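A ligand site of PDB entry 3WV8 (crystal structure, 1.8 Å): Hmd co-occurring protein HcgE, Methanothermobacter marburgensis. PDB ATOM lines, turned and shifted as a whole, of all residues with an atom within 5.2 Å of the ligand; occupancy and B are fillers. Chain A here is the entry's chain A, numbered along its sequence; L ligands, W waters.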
ATOM      1  N   VAL A  19       1.953  -2.805   6.722  1.00  0.00           N
ATOM      2  CA  VAL A  19       3.228  -2.160   6.964  1.00  0.00           C
ATOM      3  C   VAL A  19       3.515  -1.344   5.716  1.00  0.00           C
ATOM      4  O   VAL A  19       3.693  -1.800   4.526  1.00  0.00           O
ATOM      5  CB  VAL A  19       4.332  -3.227   7.024  1.00  0.00           C
ATOM      6  CG1 VAL A  19       5.667  -2.579   7.308  1.00  0.00           C
ATOM      7  CG2 VAL A  19       3.924  -4.266   8.067  1.00  0.00           C
ATOM      8  N   GLY A  20       3.663  -0.037   6.003  1.00  0.00           N
ATOM      9  CA  GLY A  20       3.761   0.997   4.967  1.00  0.00           C
ATOM     10  C   GLY A  20       2.482   1.689   4.694  1.00  0.00           C
ATOM     11  O   GLY A  20       1.517   1.043   4.311  1.00  0.00           O
ATOM     12  N   ALA A  21       2.438   3.024   4.989  1.00  0.00           N
ATOM     13  CA  ALA A  21       1.158   3.751   4.823  1.00  0.00           C
ATOM     14  C   ALA A  21       1.454   5.096   4.148  1.00  0.00           C
ATOM     15  O   ALA A  21       0.989   6.187   4.555  1.00  0.00           O
ATOM     16  CB  ALA A  21       0.491   3.932   6.238  1.00  0.00           C
ATOM     17  N   GLY A  22       2.119   4.957   2.988  1.00  0.00           N
ATOM     18  CA  GLY A  22       2.533   6.102   2.178  1.00  0.00           C
ATOM     19  C   GLY A  22       1.434   6.309   1.140  1.00  0.00           C
ATOM     20  O   GLY A  22       0.238   5.928   1.345  1.00  0.00           O
ATOM     21  N   ARG A  23       1.820   6.881   0.025  1.00  0.00           N
ATOM     22  CA  ARG A  23       0.870   7.101  -1.049  1.00  0.00           C
ATOM     23  C   ARG A  23       0.089   5.882  -1.491  1.00  0.00           C
ATOM     24  O   ARG A  23      -1.154   5.910  -1.681  1.00  0.00           O
ATOM     25  CB  ARG A  23       1.575   7.728  -2.277  1.00  0.00           C
ATOM     26  CG  ARG A  23       1.938   9.171  -2.018  1.00  0.00           C
ATOM     27  CD  ARG A  23       2.844   9.764  -3.148  1.00  0.00           C
ATOM     28  NE  ARG A  23       4.228   9.450  -2.838  1.00  0.00           N
ATOM     29  CZ  ARG A  23       5.116  10.270  -2.249  1.00  0.00           C
ATOM     30  NH1 ARG A  23       6.295   9.821  -2.011  1.00  0.00           N
ATOM     31  NH2 ARG A  23       4.875  11.533  -2.032  1.00  0.00           N
ATOM     32  N   LEU A  24       0.716   4.725  -1.474  1.00  0.00           N
ATOM     33  CA  LEU A  24      -0.024   3.458  -1.712  1.00  0.00           C
ATOM     34  C   LEU A  24      -0.762   2.900  -0.525  1.00  0.00           C
ATOM     35  O   LEU A  24      -2.023   2.659  -0.603  1.00  0.00           O
ATOM     36  CB  LEU A  24       0.928   2.416  -2.416  1.00  0.00           C
ATOM     37  CG  LEU A  24       0.253   1.038  -2.625  1.00  0.00           C
ATOM     38  CD1 LEU A  24      -0.982   0.885  -3.509  1.00  0.00           C
ATOM     39  CD2 LEU A  24       1.314   0.049  -3.181  1.00  0.00           C
ATOM     40  N   GLY A  25      -0.042   2.678   0.556  1.00  0.00           N
ATOM     41  CA  GLY A  25      -0.597   2.078   1.777  1.00  0.00           C
ATOM     42  C   GLY A  25      -1.772   2.921   2.276  1.00  0.00           C
ATOM     43  O   GLY A  25      -2.679   2.323   2.790  1.00  0.00           O
ATOM     44  N   ILE A  46       1.291   0.504  10.136  1.00  0.00           N
ATOM     45  CA  ILE A  46       2.642   0.762  10.737  1.00  0.00           C
ATOM     46  C   ILE A  46       3.562   1.503   9.756  1.00  0.00           C
ATOM     47  O   ILE A  46       3.862   0.995   8.679  1.00  0.00           O
ATOM     48  CB  ILE A  46       3.237  -0.603  11.142  1.00  0.00           C
ATOM     49  CG1 ILE A  46       2.233  -1.503  11.967  1.00  0.00           C
ATOM     50  CG2 ILE A  46       4.644  -0.499  11.799  1.00  0.00           C
ATOM     51  CD1 ILE A  46       2.776  -2.813  12.513  1.00  0.00           C
ATOM     52  N   ASP A  47       4.004   2.722  10.114  1.00  0.00           N
ATOM     53  CA  ASP A  47       4.892   3.518   9.246  1.00  0.00           C
ATOM     54  C   ASP A  47       5.539   4.603  10.126  1.00  0.00           C
ATOM     55  O   ASP A  47       4.878   5.118  11.041  1.00  0.00           O
ATOM     56  CB  ASP A  47       3.975   4.157   8.238  1.00  0.00           C
ATOM     57  CG  ASP A  47       4.780   4.788   7.066  1.00  0.00           C
ATOM     58  OD1 ASP A  47       5.822   5.502   7.301  1.00  0.00           O
ATOM     59  OD2 ASP A  47       4.398   4.572   5.898  1.00  0.00           O
ATOM     60  N   GLY A  48       6.828   4.903   9.922  1.00  0.00           N
ATOM     61  CA  GLY A  48       7.615   5.753  10.801  1.00  0.00           C
ATOM     62  C   GLY A  48       7.597   7.176  10.290  1.00  0.00           C
ATOM     63  O   GLY A  48       8.233   8.056  10.922  1.00  0.00           O
ATOM     64  N   GLN A  49       6.905   7.464   9.188  1.00  0.00           N
ATOM     65  CA  GLN A  49       7.172   8.779   8.500  1.00  0.00           C
ATOM     66  C   GLN A  49       6.062   9.745   8.723  1.00  0.00           C
ATOM     67  O   GLN A  49       4.910   9.288   8.962  1.00  0.00           O
ATOM     68  CB  GLN A  49       7.246   8.667   7.007  1.00  0.00           C
ATOM     69  CG  GLN A  49       8.567   8.170   6.552  1.00  0.00           C
ATOM     70  CD  GLN A  49       8.845   8.207   5.060  1.00  0.00           C
ATOM     71  OE1 GLN A  49       8.002   8.488   4.157  1.00  0.00           O
ATOM     72  NE2 GLN A  49      10.062   7.797   4.782  1.00  0.00           N
ATOM     73  N   ASP A  55       3.153  15.291   0.244  1.00  0.00           N
ATOM     74  CA  ASP A  55       2.000  14.352   0.454  1.00  0.00           C
ATOM     75  C   ASP A  55       0.635  14.942   0.195  1.00  0.00           C
ATOM     76  O   ASP A  55      -0.188  14.998   1.080  1.00  0.00           O
ATOM     77  CB  ASP A  55       2.084  13.763   1.873  1.00  0.00           C
ATOM     78  CG  ASP A  55       3.254  12.805   2.010  1.00  0.00           C
ATOM     79  OD1 ASP A  55       3.582  12.100   1.018  1.00  0.00           O
ATOM     80  OD2 ASP A  55       3.916  12.786   3.042  1.00  0.00           O
ATOM     81  N   LYS A  69       1.766  10.058   9.455  1.00  0.00           N
ATOM     82  CA  LYS A  69       0.848   9.246   8.618  1.00  0.00           C
ATOM     83  C   LYS A  69      -0.137   8.354   9.379  1.00  0.00           C
ATOM     84  O   LYS A  69      -1.382   8.453   9.189  1.00  0.00           O
ATOM     85  CB  LYS A  69       1.667   8.532   7.498  1.00  0.00           C
ATOM     86  CG  LYS A  69       2.319   9.482   6.539  1.00  0.00           C
ATOM     87  CD  LYS A  69       3.248   8.758   5.574  1.00  0.00           C
ATOM     88  CE  LYS A  69       4.099   9.751   4.835  1.00  0.00           C
ATOM     89  NZ  LYS A  69       4.994   9.125   3.828  1.00  0.00           N
ATOM     90  N   GLU A  90       6.098   3.686  13.708  1.00  0.00           N
ATOM     91  CA  GLU A  90       7.487   3.246  13.706  1.00  0.00           C
ATOM     92  C   GLU A  90       7.784   2.569  12.430  1.00  0.00           C
ATOM     93  O   GLU A  90       6.847   1.967  11.863  1.00  0.00           O
ATOM     94  CB  GLU A  90       7.786   2.292  14.834  1.00  0.00           C
ATOM     95  CG  GLU A  90       7.530   2.935  16.243  1.00  0.00           C
ATOM     96  CD  GLU A  90       7.821   1.931  17.364  1.00  0.00           C
ATOM     97  OE1 GLU A  90       7.820   0.714  17.091  1.00  0.00           O
ATOM     98  OE2 GLU A  90       8.067   2.297  18.532  1.00  0.00           O
ATOM     99  N   TYR A  91       9.042   2.635  12.006  1.00  0.00           N
ATOM    100  CA  TYR A  91       9.479   1.701  10.934  1.00  0.00           C
ATOM    101  C   TYR A  91       9.560   0.210  11.431  1.00  0.00           C
ATOM    102  O   TYR A  91       9.951  -0.040  12.597  1.00  0.00           O
ATOM    103  CB  TYR A  91      10.802   2.146  10.306  1.00  0.00           C
ATOM    104  CG  TYR A  91      10.749   3.470   9.625  1.00  0.00           C
ATOM    105  CD1 TYR A  91       9.979   3.691   8.473  1.00  0.00           C
ATOM    106  CD2 TYR A  91      11.313   4.616  10.258  1.00  0.00           C
ATOM    107  CE1 TYR A  91       9.928   4.943   7.891  1.00  0.00           C
ATOM    108  CE2 TYR A  91      11.272   5.875   9.725  1.00  0.00           C
ATOM    109  CZ  TYR A  91      10.583   6.078   8.552  1.00  0.00           C
ATOM    110  OH  TYR A  91      10.589   7.424   8.288  1.00  0.00           O
ATOM    111  N   ILE A  92       9.241  -0.819  10.608  1.00  0.00           N
ATOM    112  CA  ILE A  92       9.617  -2.207  11.041  1.00  0.00           C
ATOM    113  C   ILE A  92      11.088  -2.451  10.763  1.00  0.00           C
ATOM    114  O   ILE A  92      11.626  -2.156   9.619  1.00  0.00           O
ATOM    115  CB  ILE A  92       8.758  -3.258  10.302  1.00  0.00           C
ATOM    116  CG1 ILE A  92       7.269  -3.065  10.728  1.00  0.00           C
ATOM    117  CG2 ILE A  92       9.267  -4.710  10.396  1.00  0.00           C
ATOM    118  CD1 ILE A  92       6.934  -3.670  12.105  1.00  0.00           C
ATOM    119  N   GLU A 108       3.647  -2.656   1.864  1.00  0.00           N
ATOM    120  CA  GLU A 108       3.614  -1.599   0.829  1.00  0.00           C
ATOM    121  C   GLU A 108       4.599  -0.471   1.214  1.00  0.00           C
ATOM    122  O   GLU A 108       4.185   0.615   1.600  1.00  0.00           O
ATOM    123  CB  GLU A 108       2.159  -1.013   0.640  1.00  0.00           C
ATOM    124  CG  GLU A 108       1.137  -2.000   0.044  1.00  0.00           C
ATOM    125  CD  GLU A 108      -0.277  -1.662   0.300  1.00  0.00           C
ATOM    126  OE1 GLU A 108      -0.671  -1.314   1.504  1.00  0.00           O
ATOM    127  OE2 GLU A 108      -1.023  -1.554  -0.668  1.00  0.00           O
ATOM    128  N   ILE A 109       5.853  -0.803   1.283  1.00  0.00           N
ATOM    129  CA  ILE A 109       6.906   0.144   1.738  1.00  0.00           C
ATOM    130  C   ILE A 109       7.701   0.527   0.516  1.00  0.00           C
ATOM    131  O   ILE A 109       7.812  -0.250  -0.597  1.00  0.00           O
ATOM    132  CB  ILE A 109       7.786  -0.560   2.753  1.00  0.00           C
ATOM    133  CG1 ILE A 109       8.443  -1.968   2.260  1.00  0.00           C
ATOM    134  CG2 ILE A 109       6.886  -0.820   4.033  1.00  0.00           C
ATOM    135  CD1 ILE A 109       9.646  -2.497   3.198  1.00  0.00           C
ATOM    136  N   ALA A 110       8.336   1.670   0.661  1.00  0.00           N
ATOM    137  CA  ALA A 110       9.205   2.197  -0.406  1.00  0.00           C
ATOM    138  C   ALA A 110      10.253   3.009   0.268  1.00  0.00           C
ATOM    139  O   ALA A 110      10.042   3.534   1.373  1.00  0.00           O
ATOM    140  CB  ALA A 110       8.350   3.023  -1.357  1.00  0.00           C
ATOM    141  N   GLY A 111      11.453   3.038  -0.319  1.00  0.00           N
ATOM    142  CA  GLY A 111      12.437   3.960   0.129  1.00  0.00           C
ATOM    143  C   GLY A 111      13.564   3.056   0.578  1.00  0.00           C
ATOM    144  O   GLY A 111      13.377   2.253   1.494  1.00  0.00           O
ATOM    145  N   THR A 114      14.382  -2.091   0.559  1.00  0.00           N
ATOM    146  CA  THR A 114      13.296  -2.696   1.230  1.00  0.00           C
ATOM    147  C   THR A 114      13.227  -4.220   1.161  1.00  0.00           C
ATOM    148  O   THR A 114      12.448  -4.757   1.916  1.00  0.00           O
ATOM    149  CB  THR A 114      11.985  -2.209   0.610  1.00  0.00           C
ATOM    150  OG1 THR A 114      12.031  -2.372  -0.819  1.00  0.00           O
ATOM    151  CG2 THR A 114      11.774  -0.711   0.891  1.00  0.00           C
ATOM    152  N   ILE A 117      14.134  -6.340   4.653  1.00  0.00           N
ATOM    153  CA  ILE A 117      12.989  -6.213   5.637  1.00  0.00           C
ATOM    154  C   ILE A 117      11.624  -6.861   5.254  1.00  0.00           C
ATOM    155  O   ILE A 117      10.952  -7.564   6.079  1.00  0.00           O
ATOM    156  CB  ILE A 117      12.820  -4.750   6.236  1.00  0.00           C
ATOM    157  CG1 ILE A 117      12.056  -4.892   7.544  1.00  0.00           C
ATOM    158  CG2 ILE A 117      12.121  -3.812   5.264  1.00  0.00           C
ATOM    159  CD1 ILE A 117      12.911  -5.498   8.701  1.00  0.00           C
ATOM    160  N   VAL A 138       5.310  -0.825  -8.610  1.00  0.00           N
ATOM    161  CA  VAL A 138       4.094   0.032  -8.719  1.00  0.00           C
ATOM    162  C   VAL A 138       4.345   1.249  -9.634  1.00  0.00           C
ATOM    163  O   VAL A 138       3.517   2.192  -9.701  1.00  0.00           O
ATOM    164  CB  VAL A 138       3.539   0.408  -7.310  1.00  0.00           C
ATOM    165  CG1 VAL A 138       3.443  -0.915  -6.481  1.00  0.00           C
ATOM    166  CG2 VAL A 138       4.439   1.447  -6.614  1.00  0.00           C
ATOM    167  N   VAL A 187       5.748   7.155 -10.831  1.00  0.00           N
ATOM    168  CA  VAL A 187       4.519   6.629 -10.202  1.00  0.00           C
ATOM    169  C   VAL A 187       3.405   7.695 -10.290  1.00  0.00           C
ATOM    170  O   VAL A 187       3.602   8.777  -9.763  1.00  0.00           O
ATOM    171  CB  VAL A 187       4.885   6.249  -8.740  1.00  0.00           C
ATOM    172  CG1 VAL A 187       3.706   5.704  -7.978  1.00  0.00           C
ATOM    173  CG2 VAL A 187       5.949   5.167  -8.766  1.00  0.00           C
ATOM    174  N   LEU A 192      -1.520   4.003  -8.723  1.00  0.00           N
ATOM    175  CA  LEU A 192      -1.666   3.666  -7.296  1.00  0.00           C
ATOM    176  C   LEU A 192      -3.124   3.351  -6.844  1.00  0.00           C
ATOM    177  O   LEU A 192      -3.345   2.391  -6.055  1.00  0.00           O
ATOM    178  CB  LEU A 192      -1.079   4.755  -6.366  1.00  0.00           C
ATOM    179  CG  LEU A 192       0.414   4.951  -6.586  1.00  0.00           C
ATOM    180  CD1 LEU A 192       0.924   5.972  -5.564  1.00  0.00           C
ATOM    181  CD2 LEU A 192       1.158   3.649  -6.166  1.00  0.00           C
HETATM  182  P1  LIG L   1       5.062   5.874  -4.683  1.00  0.00           P
HETATM  183  O1  LIG L   1       4.851   4.630  -5.613  1.00  0.00           O
HETATM  184  O2  LIG L   1       6.501   6.171  -4.202  1.00  0.00           O
HETATM  185  O3  LIG L   1       4.389   7.179  -5.031  1.00  0.00           O
HETATM  186  P2  LIG L   1       4.557   4.522  -2.205  1.00  0.00           P
HETATM  187  O4  LIG L   1       5.225   3.326  -2.740  1.00  0.00           O
HETATM  188  O5  LIG L   1       3.397   4.507  -1.335  1.00  0.00           O
HETATM  189  O6  LIG L   1       4.081   5.391  -3.439  1.00  0.00           O
HETATM  190  P3  LIG L   1       5.738   6.509  -0.467  1.00  0.00           P
HETATM  191  O7  LIG L   1       7.096   7.094  -0.303  1.00  0.00           O
HETATM  192  O8  LIG L   1       4.628   7.498  -0.604  1.00  0.00           O
HETATM  193  O9  LIG L   1       5.721   5.437  -1.616  1.00  0.00           O
HETATM  194  O10 LIG L   1       5.457   5.566   0.796  1.00  0.00           O
HETATM  195  C1  LIG L   1       6.398   4.563   1.195  1.00  0.00           C
HETATM  196  C2  LIG L   1       6.145   4.398   2.743  1.00  0.00           C
HETATM  197  O11 LIG L   1       6.775   3.170   3.198  1.00  0.00           O
HETATM  198  C3  LIG L   1       6.667   5.599   3.518  1.00  0.00           C
HETATM  199  O12 LIG L   1       5.544   6.173   4.298  1.00  0.00           O
HETATM  200  C4  LIG L   1       7.628   4.863   4.427  1.00  0.00           C
HETATM  201  O13 LIG L   1       7.643   5.503   5.723  1.00  0.00           O
HETATM  202  C5  LIG L   1       7.204   3.479   4.543  1.00  0.00           C
HETATM  203  N1  LIG L   1       8.330   2.603   4.907  1.00  0.00           N
HETATM  204  C6  LIG L   1       9.517   2.455   4.297  1.00  0.00           C
HETATM  205  N2  LIG L   1      10.206   1.504   4.916  1.00  0.00           N
HETATM  206  C7  LIG L   1       9.483   1.075   6.018  1.00  0.00           C
HETATM  207  C8  LIG L   1       9.521   0.139   7.089  1.00  0.00           C
HETATM  208  N3  LIG L   1      10.666  -0.467   7.327  1.00  0.00           N
HETATM  209  N4  LIG L   1       8.435   0.028   7.973  1.00  0.00           N
HETATM  210  C9  LIG L   1       7.343   0.805   7.835  1.00  0.00           C
HETATM  211  N5  LIG L   1       7.229   1.639   6.891  1.00  0.00           N
HETATM  212  C10 LIG L   1       8.270   1.854   6.014  1.00  0.00           C
HETATM  213  O   HOH W   1       3.386   8.703  -7.147  1.00  0.00           O
HETATM  214  O   HOH W   2       2.935   3.079   1.064  1.00  0.00           O
HETATM  215  O   HOH W   3       6.967   3.049  -4.708  1.00  0.00           O
HETATM  216  O   HOH W   4       7.722   9.215   1.536  1.00  0.00           O
HETATM  217  O   HOH W   5       6.875   8.563  -4.024  1.00  0.00           O
HETATM  218  O   HOH W   6       3.775   9.304   1.461  1.00  0.00           O
HETATM  219  O   HOH W   7       9.533   6.733   1.632  1.00  0.00           O
HETATM  220  O   HOH W   8      12.519  -0.041   4.004  1.00  0.00           O
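N of Gln 49 sits at hydrogen-bond distance from OD1 of Asp 47. The side-chain amino group (NZ) of Lys 69 lies within salt-bridge range of the side-chain carboxylate (OD2) of Asp 55 (3.9 Å). The backbone NH (N) of Gly 20 is in hydrogen-bond range of the backbone carbonyl oxygen (O) of Ile 46 (2.9 Å). The side-chain carboxylate (OD1) of Asp 55 lies within salt-bridge range of the guanidinium group (NH2) of Arg 23 (3.4 Å). OE1 of Gln 49 lies within hydrogen-bond range of NZ of Lys 69. OD2 of Asp 47 is in hydrogen-bond range of N of Ala 21, at 2.7 Å. The backbone carbonyl oxygen (O) of Val 19 lies within hydrogen-bond range of the backbone NH (N) of Glu 108, 2.8 Å away. The backbone carbonyl oxygen of Asp 47 is in hydrogen-bond range of the backbone NH of Glu 90 (3.3 Å).
Water W5 bridges an oxygen (O2) of the ligand (2.4 Å) and the guanidinium group (NH1) of Arg 23 (2.4 Å). Water W1 lies within hydrogen-bond range of the backbone carbonyl oxygen of Val 187 (2.6 Å) and an oxygen (O3) of the ligand (2.8 Å). Water W2 lies within hydrogen-bond range of the backbone NH of Gly 22, the backbone carbonyl oxygen of Glu 108, an oxygen (O5) of the ligand and the backbone NH of Gly 25. Water W6 lies within hydrogen-bond range of the side-chain amino group of Lys 69 (2.7 Å), the side-chain carboxylate of Asp 55 (2.8 Å), an oxygen (O8) of the ligand (2.9 Å) and the backbone NH of Arg 23 (3.4 Å). Water W4 bridges OE1 of Gln 49 (2.7 Å) and O7 of the ligand (2.9 Å). Water W7 lies within hydrogen-bond range of an oxygen (O7) of the ligand (3.1 Å), the backbone carbonyl oxygen of Ala 110 (3.2 Å) and the side-chain amide nitrogen of Gln 49 (3.4 Å).
OE1 of Gln 49 sits close to O12 of the ligand (3.4 Å). The side-chain carboxylate (OD1) of Asp 47 sits at hydrogen-bond distance from an oxygen (O13) of the ligand, 2.4 Å away. The guanidinium group of Arg 23 lies within salt-bridge range of an oxygen (O8) of the ligand (3.0 Å). N of Ile 92 sits at hydrogen-bond distance from N4 of the ligand (2.9 Å). O of Ile 92 lies within hydrogen-bond range of N3 of the ligand (3.0 Å). The side-chain amino group (NZ) of Lys 69 is in hydrogen-bond range of an oxygen (O12) of the ligand, 3.0 Å away. The backbone NH (N) of Ala 110 is in hydrogen-bond range of an oxygen (O11) of the ligand (3.3 Å). N of Arg 23 sits at hydrogen-bond distance from O8 of the ligand. The backbone NH (N) of Leu 24 sits at hydrogen-bond distance from an oxygen (O5) of the ligand (2.7 Å).
Val 19 touches the ligand. CA of Gly 22 touches O10 of the ligand, 3.3 Å away. Ile 46 touches the ligand. Tyr 91 touches the ligand (CE1 to O13, 3.2 Å). O of Glu 108 touches O11 of the ligand, at 3.97 Å. Ile 109 touches the ligand (CA to O11, 3.4 Å). Val 138 touches the ligand (CG2 to O1, 3.4 Å). Val 187 touches the ligand. CD1 of Leu 192 touches O3 of the ligand (3.7 Å). 16 residues have an atom within 4 Å of the ligand: Val 19, Gly 22, Arg 23, Leu 24, Ile 46, Asp 47, Gln 49, Lys 69, Tyr 91, Ile 92, Glu 108, Ile 109, Ala 110, Val 138, Val 187 and Leu 192. The nearest printed residue that does not touch the ligand is Gly 20 (4.02 Å).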
